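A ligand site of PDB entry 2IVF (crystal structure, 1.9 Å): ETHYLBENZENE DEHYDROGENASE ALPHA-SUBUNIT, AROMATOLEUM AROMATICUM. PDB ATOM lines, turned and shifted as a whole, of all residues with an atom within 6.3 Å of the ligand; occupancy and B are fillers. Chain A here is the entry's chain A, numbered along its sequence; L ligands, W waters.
A ring nitrogen (ND1) of His 82 is bound to an iron atom (FE3) of the ligand, at 2.2 Å. The backbone NH (N) of Cys 92 lies close to a sulfur (S1) of the ligand (3.8 Å). The side-chain sulfur of Cys 92 is bound to an iron atom (FE2) of the ligand (2.2 Å). SG of Cys 86 is bound to FE4 of the ligand (2.3 Å). The backbone NH (N) of Cys 127 lies close to a sulfur (S4) of the ligand, 3.4 Å away. FE1 of the ligand is bound by SG of Cys 127 (2.3 Å). A sulfur (S2) of the ligand sits close to the side-chain amide nitrogen (ND2) of Asn 84 (3.4 Å). The backbone NH (N) of Ser 91 lies close to a sulfur (S1) of the ligand, at 3.7 Å.
O of Cys 92 sits at hydrogen-bond distance from OG of Ser 81, 2.6 Å away. SG of Cys 92 sits close to O of Gly 90, at 3.6 Å. The side-chain sulfur of Cys 86 sits close to the backbone NH of Gly 90 (3.3 Å). The side-chain sulfur (SG) of Cys 127 sits close to the backbone NH (N) of Gly 130 (3.5 Å). The side-chain sulfur of Cys 127 lies close to the backbone NH of Lys 129 (3.5 Å). The backbone carbonyl oxygen (O) of Asn 84 is in hydrogen-bond range of the side-chain amide nitrogen (NE2) of Gln 89, at 3.0 Å. The side-chain amide oxygen of Gln 89 lies within hydrogen-bond range of the backbone NH of Ser 91 (2.9 Å). ND1 of His 858 lies within hydrogen-bond range of N of Ile 854 (3.0 Å).
OG of Ser 81 touches S1 of the ligand, 3.9 Å away. Gly 90 touches the ligand. Phe 94 touches the ligand. Gly 126 touches the ligand (CA to S4, 3.6 Å). Gly 130 touches the ligand. Ile 854 touches the ligand. Hydrophobic or aromatic side chains that line the ligand: His 82, Phe 94 and Ile 854. 12 residues have an atom within 4 Å of the ligand: Ser 81, His 82, Asn 84, Cys 86, Gly 90, Ser 91, Cys 92, Phe 94, Gly 126, Cys 127, Gly 130 and Ile 854.
Water W1 lies within hydrogen-bond range of the side-chain hydroxyl (OG) of Ser 263 and a sulfur (S3) of the ligand.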
ATOM      1  N   SER A  81      15.619  26.014   4.613  1.00  0.00           N
ATOM      2  CA  SER A  81      15.905  24.603   4.600  1.00  0.00           C
ATOM      3  C   SER A  81      16.359  24.245   6.032  1.00  0.00           C
ATOM      4  O   SER A  81      16.279  25.108   6.938  1.00  0.00           O
ATOM      5  CB  SER A  81      16.971  24.208   3.567  1.00  0.00           C
ATOM      6  OG  SER A  81      16.919  22.821   3.317  1.00  0.00           O
ATOM      7  N   HIS A  82      16.787  22.998   6.225  1.00  0.00           N
ATOM      8  CA  HIS A  82      17.141  22.461   7.550  1.00  0.00           C
ATOM      9  C   HIS A  82      18.597  21.984   7.549  1.00  0.00           C
ATOM     10  O   HIS A  82      19.034  21.382   6.603  1.00  0.00           O
ATOM     11  CB  HIS A  82      16.110  21.376   7.872  1.00  0.00           C
ATOM     12  CG  HIS A  82      14.721  21.760   7.444  1.00  0.00           C
ATOM     13  ND1 HIS A  82      14.067  21.201   6.357  1.00  0.00           N
ATOM     14  CD2 HIS A  82      13.917  22.758   7.879  1.00  0.00           C
ATOM     15  CE1 HIS A  82      12.915  21.822   6.168  1.00  0.00           C
ATOM     16  NE2 HIS A  82      12.784  22.757   7.099  1.00  0.00           N
ATOM     17  N   LEU A  83      19.357  22.306   8.600  1.00  0.00           N
ATOM     18  CA  LEU A  83      20.781  22.039   8.602  1.00  0.00           C
ATOM     19  C   LEU A  83      21.105  20.715   9.283  1.00  0.00           C
ATOM     20  O   LEU A  83      22.201  20.209   9.126  1.00  0.00           O
ATOM     21  CB  LEU A  83      21.534  23.190   9.249  1.00  0.00           C
ATOM     22  CG  LEU A  83      21.477  24.515   8.463  1.00  0.00           C
ATOM     23  CD1 LEU A  83      21.522  24.347   6.941  1.00  0.00           C
ATOM     24  CD2 LEU A  83      20.239  25.287   8.827  1.00  0.00           C
ATOM     25  N   ASN A  84      20.127  20.145   9.992  1.00  0.00           N
ATOM     26  CA  ASN A  84      20.189  18.773  10.510  1.00  0.00           C
ATOM     27  C   ASN A  84      20.674  17.861   9.433  1.00  0.00           C
ATOM     28  O   ASN A  84      20.334  17.986   8.309  1.00  0.00           O
ATOM     29  CB  ASN A  84      18.871  18.292  11.176  1.00  0.00           C
ATOM     30  CG  ASN A  84      17.619  18.396  10.321  1.00  0.00           C
ATOM     31  OD1 ASN A  84      16.486  18.535  10.859  1.00  0.00           O
ATOM     32  ND2 ASN A  84      17.764  18.325   8.979  1.00  0.00           N
ATOM     33  N   ILE A  85      21.587  16.966   9.785  1.00  0.00           N
ATOM     34  CA  ILE A  85      22.123  16.073   8.781  1.00  0.00           C
ATOM     35  C   ILE A  85      21.219  14.875   8.530  1.00  0.00           C
ATOM     36  O   ILE A  85      21.413  13.778   9.027  1.00  0.00           O
ATOM     37  CB  ILE A  85      23.594  15.672   9.062  1.00  0.00           C
ATOM     38  CG1 ILE A  85      24.487  16.934   9.112  1.00  0.00           C
ATOM     39  CG2 ILE A  85      24.104  14.739   7.964  1.00  0.00           C
ATOM     40  CD1 ILE A  85      24.391  17.855   7.810  1.00  0.00           C
ATOM     41  N   CYS A  86      20.166  15.113   7.738  1.00  0.00           N
ATOM     42  CA  CYS A  86      19.637  14.039   6.927  1.00  0.00           C
ATOM     43  C   CYS A  86      20.744  13.666   5.969  1.00  0.00           C
ATOM     44  O   CYS A  86      21.598  14.498   5.659  1.00  0.00           O
ATOM     45  CB  CYS A  86      18.367  14.487   6.206  1.00  0.00           C
ATOM     46  SG  CYS A  86      18.463  16.234   5.618  1.00  0.00           S
ATOM     47  N   PRO A  88      21.425  11.021   2.356  1.00  0.00           N
ATOM     48  CA  PRO A  88      22.066  12.174   1.724  1.00  0.00           C
ATOM     49  C   PRO A  88      21.336  13.425   2.156  1.00  0.00           C
ATOM     50  O   PRO A  88      20.119  13.376   2.313  1.00  0.00           O
ATOM     51  CB  PRO A  88      21.881  11.890   0.250  1.00  0.00           C
ATOM     52  CG  PRO A  88      21.919  10.429   0.145  1.00  0.00           C
ATOM     53  CD  PRO A  88      21.175   9.933   1.370  1.00  0.00           C
ATOM     54  N   GLN A  89      22.062  14.514   2.399  1.00  0.00           N
ATOM     55  CA  GLN A  89      21.384  15.713   2.924  1.00  0.00           C
ATOM     56  C   GLN A  89      20.322  16.129   1.935  1.00  0.00           C
ATOM     57  O   GLN A  89      20.603  16.250   0.766  1.00  0.00           O
ATOM     58  CB  GLN A  89      22.388  16.822   3.190  1.00  0.00           C
ATOM     59  CG  GLN A  89      22.159  17.573   4.491  1.00  0.00           C
ATOM     60  CD  GLN A  89      21.134  18.661   4.344  1.00  0.00           C
ATOM     61  OE1 GLN A  89      20.919  19.176   3.243  1.00  0.00           O
ATOM     62  NE2 GLN A  89      20.471  19.029   5.456  1.00  0.00           N
ATOM     63  N   GLY A  90      19.083  16.348   2.390  1.00  0.00           N
ATOM     64  CA  GLY A  90      18.023  16.556   1.411  1.00  0.00           C
ATOM     65  C   GLY A  90      18.197  17.849   0.639  1.00  0.00           C
ATOM     66  O   GLY A  90      17.823  17.941  -0.548  1.00  0.00           O
ATOM     67  N   SER A  91      18.733  18.864   1.305  1.00  0.00           N
ATOM     68  CA  SER A  91      18.971  20.197   0.744  1.00  0.00           C
ATOM     69  C   SER A  91      17.722  20.676   0.057  1.00  0.00           C
ATOM     70  O   SER A  91      17.766  21.256  -1.036  1.00  0.00           O
ATOM     71  CB  SER A  91      20.136  20.281  -0.276  1.00  0.00           C
ATOM     72  OG  SER A  91      21.328  20.077   0.387  1.00  0.00           O
ATOM     73  N   CYS A  92      16.622  20.441   0.738  1.00  0.00           N
ATOM     74  CA  CYS A  92      15.319  20.776   0.229  1.00  0.00           C
ATOM     75  C   CYS A  92      15.021  22.222   0.421  1.00  0.00           C
ATOM     76  O   CYS A  92      15.068  22.697   1.554  1.00  0.00           O
ATOM     77  CB  CYS A  92      14.287  19.970   1.007  1.00  0.00           C
ATOM     78  SG  CYS A  92      14.623  18.243   1.137  1.00  0.00           S
ATOM     79  N   PHE A  94      12.645  25.275   0.779  1.00  0.00           N
ATOM     80  CA  PHE A  94      11.290  25.598   1.219  1.00  0.00           C
ATOM     81  C   PHE A  94      10.994  27.060   1.145  1.00  0.00           C
ATOM     82  O   PHE A  94      11.866  27.915   1.307  1.00  0.00           O
ATOM     83  CB  PHE A  94      11.070  25.181   2.660  1.00  0.00           C
ATOM     84  CG  PHE A  94      10.805  23.708   2.847  1.00  0.00           C
ATOM     85  CD1 PHE A  94      11.773  22.807   2.637  1.00  0.00           C
ATOM     86  CD2 PHE A  94       9.540  23.251   3.190  1.00  0.00           C
ATOM     87  CE1 PHE A  94      11.559  21.475   2.810  1.00  0.00           C
ATOM     88  CE2 PHE A  94       9.305  21.915   3.365  1.00  0.00           C
ATOM     89  CZ  PHE A  94      10.317  21.023   3.160  1.00  0.00           C
ATOM     90  N   LEU A 125      10.916  17.317  -3.345  1.00  0.00           N
ATOM     91  CA  LEU A 125      11.812  17.163  -2.206  1.00  0.00           C
ATOM     92  C   LEU A 125      11.027  17.261  -0.901  1.00  0.00           C
ATOM     93  O   LEU A 125       9.791  17.209  -0.914  1.00  0.00           O
ATOM     94  CB  LEU A 125      12.977  18.196  -2.238  1.00  0.00           C
ATOM     95  CG  LEU A 125      13.995  18.046  -3.394  1.00  0.00           C
ATOM     96  CD1 LEU A 125      14.851  19.310  -3.452  1.00  0.00           C
ATOM     97  CD2 LEU A 125      14.822  16.717  -3.265  1.00  0.00           C
ATOM     98  N   GLY A 126      11.743  17.354   0.218  1.00  0.00           N
ATOM     99  CA  GLY A 126      11.106  17.533   1.497  1.00  0.00           C
ATOM    100  C   GLY A 126      10.837  16.242   2.247  1.00  0.00           C
ATOM    101  O   GLY A 126      11.007  15.118   1.746  1.00  0.00           O
ATOM    102  N   CYS A 127      10.465  16.438   3.510  1.00  0.00           N
ATOM    103  CA  CYS A 127      10.044  15.356   4.375  1.00  0.00           C
ATOM    104  C   CYS A 127       9.150  15.902   5.462  1.00  0.00           C
ATOM    105  O   CYS A 127       8.912  17.143   5.546  1.00  0.00           O
ATOM    106  CB  CYS A 127      11.214  14.661   4.959  1.00  0.00           C
ATOM    107  SG  CYS A 127      11.988  15.468   6.405  1.00  0.00           S
ATOM    108  N   GLN A 128       8.657  15.005   6.296  1.00  0.00           N
ATOM    109  CA  GLN A 128       7.624  15.419   7.253  1.00  0.00           C
ATOM    110  C   GLN A 128       8.227  16.259   8.415  1.00  0.00           C
ATOM    111  O   GLN A 128       7.553  17.107   8.992  1.00  0.00           O
ATOM    112  CB  GLN A 128       6.795  14.213   7.757  1.00  0.00           C
ATOM    113  CG  GLN A 128       7.512  13.317   8.817  1.00  0.00           C
ATOM    114  CD  GLN A 128       8.575  12.410   8.234  1.00  0.00           C
ATOM    115  OE1 GLN A 128       9.261  12.775   7.256  1.00  0.00           O
ATOM    116  NE2 GLN A 128       8.779  11.256   8.850  1.00  0.00           N
ATOM    117  N   LYS A 129       9.498  16.025   8.730  1.00  0.00           N
ATOM    118  CA  LYS A 129      10.128  16.756   9.795  1.00  0.00           C
ATOM    119  C   LYS A 129      10.343  18.180   9.304  1.00  0.00           C
ATOM    120  O   LYS A 129       9.982  19.117   9.992  1.00  0.00           O
ATOM    121  CB  LYS A 129      11.455  16.136  10.161  1.00  0.00           C
ATOM    122  CG  LYS A 129      11.338  14.881  11.003  1.00  0.00           C
ATOM    123  CD  LYS A 129      11.087  13.626  10.153  1.00  0.00           C
ATOM    124  CE  LYS A 129      12.276  13.272   9.256  1.00  0.00           C
ATOM    125  NZ  LYS A 129      11.963  12.094   8.380  1.00  0.00           N
ATOM    126  N   GLY A 130      10.908  18.310   8.108  1.00  0.00           N
ATOM    127  CA  GLY A 130      11.149  19.630   7.478  1.00  0.00           C
ATOM    128  C   GLY A 130       9.890  20.425   7.263  1.00  0.00           C
ATOM    129  O   GLY A 130       9.840  21.646   7.485  1.00  0.00           O
ATOM    130  N   SER A 131       8.849  19.718   6.821  1.00  0.00           N
ATOM    131  CA  SER A 131       7.564  20.339   6.471  1.00  0.00           C
ATOM    132  C   SER A 131       6.734  20.723   7.707  1.00  0.00           C
ATOM    133  O   SER A 131       5.636  21.313   7.548  1.00  0.00           O
ATOM    134  CB  SER A 131       6.782  19.383   5.564  1.00  0.00           C
ATOM    135  OG  SER A 131       7.428  19.228   4.311  1.00  0.00           O
ATOM    136  N   PRO A 262      13.713  10.178   2.363  1.00  0.00           N
ATOM    137  CA  PRO A 262      12.379  10.418   1.799  1.00  0.00           C
ATOM    138  C   PRO A 262      12.347  11.451   0.708  1.00  0.00           C
ATOM    139  O   PRO A 262      11.491  11.371  -0.137  1.00  0.00           O
ATOM    140  CB  PRO A 262      11.553  10.857   2.997  1.00  0.00           C
ATOM    141  CG  PRO A 262      12.548  11.382   4.017  1.00  0.00           C
ATOM    142  CD  PRO A 262      13.802  10.574   3.778  1.00  0.00           C
ATOM    143  N   SER A 263      13.308  12.387   0.688  1.00  0.00           N
ATOM    144  CA  SER A 263      13.301  13.424  -0.345  1.00  0.00           C
ATOM    145  C   SER A 263      13.553  12.833  -1.712  1.00  0.00           C
ATOM    146  O   SER A 263      13.106  13.425  -2.692  1.00  0.00           O
ATOM    147  CB  SER A 263      14.309  14.550  -0.093  1.00  0.00           C
ATOM    148  OG  SER A 263      15.625  14.082  -0.032  1.00  0.00           O
ATOM    149  N   THR A 662      22.904  24.632   3.143  1.00  0.00           N
ATOM    150  CA  THR A 662      22.905  23.199   3.392  1.00  0.00           C
ATOM    151  C   THR A 662      24.245  22.575   2.956  1.00  0.00           C
ATOM    152  O   THR A 662      25.090  23.239   2.387  1.00  0.00           O
ATOM    153  CB  THR A 662      21.764  22.556   2.665  1.00  0.00           C
ATOM    154  OG1 THR A 662      21.873  22.868   1.281  1.00  0.00           O
ATOM    155  CG2 THR A 662      20.443  23.086   3.204  1.00  0.00           C
ATOM    156  N   ILE A 854      15.030  13.821  12.478  1.00  0.00           N
ATOM    157  CA  ILE A 854      16.402  13.851  11.974  1.00  0.00           C
ATOM    158  C   ILE A 854      17.273  13.836  13.268  1.00  0.00           C
ATOM    159  O   ILE A 854      17.338  14.825  14.041  1.00  0.00           O
ATOM    160  CB  ILE A 854      16.718  15.049  11.061  1.00  0.00           C
ATOM    161  CG1 ILE A 854      15.734  15.083   9.877  1.00  0.00           C
ATOM    162  CG2 ILE A 854      18.115  14.986  10.549  1.00  0.00           C
ATOM    163  CD1 ILE A 854      15.789  13.820   8.930  1.00  0.00           C
ATOM    164  N   HIS A 858      13.928  16.373  16.386  1.00  0.00           N
ATOM    165  CA  HIS A 858      12.463  16.380  16.456  1.00  0.00           C
ATOM    166  C   HIS A 858      11.916  15.346  17.448  1.00  0.00           C
ATOM    167  O   HIS A 858      10.658  15.156  17.579  1.00  0.00           O
ATOM    168  CB  HIS A 858      11.873  16.082  15.092  1.00  0.00           C
ATOM    169  CG  HIS A 858      12.517  16.826  13.982  1.00  0.00           C
ATOM    170  ND1 HIS A 858      13.638  16.376  13.338  1.00  0.00           N
ATOM    171  CD2 HIS A 858      12.212  18.016  13.410  1.00  0.00           C
ATOM    172  CE1 HIS A 858      14.019  17.260  12.424  1.00  0.00           C
ATOM    173  NE2 HIS A 858      13.138  18.245  12.411  1.00  0.00           N
HETATM  174 FE1  LIG L   1      13.675  16.779   5.535  1.00  0.00          FE
HETATM  175 FE2  LIG L   1      14.760  17.927   3.332  1.00  0.00          FE
HETATM  176 FE3  LIG L   1      14.722  19.278   5.624  1.00  0.00          FE
HETATM  177 FE4  LIG L   1      16.380  17.107   5.354  1.00  0.00          FE
HETATM  178  S1  LIG L   1      16.584  19.088   4.277  1.00  0.00           S
HETATM  179  S2  LIG L   1      14.983  17.635   7.169  1.00  0.00           S
HETATM  180  S3  LIG L   1      15.071  15.812   3.987  1.00  0.00           S
HETATM  181  S4  LIG L   1      12.871  18.638   4.413  1.00  0.00           S
HETATM  182  O   HOH W   1      15.709  13.116   2.404  1.00  0.00           O
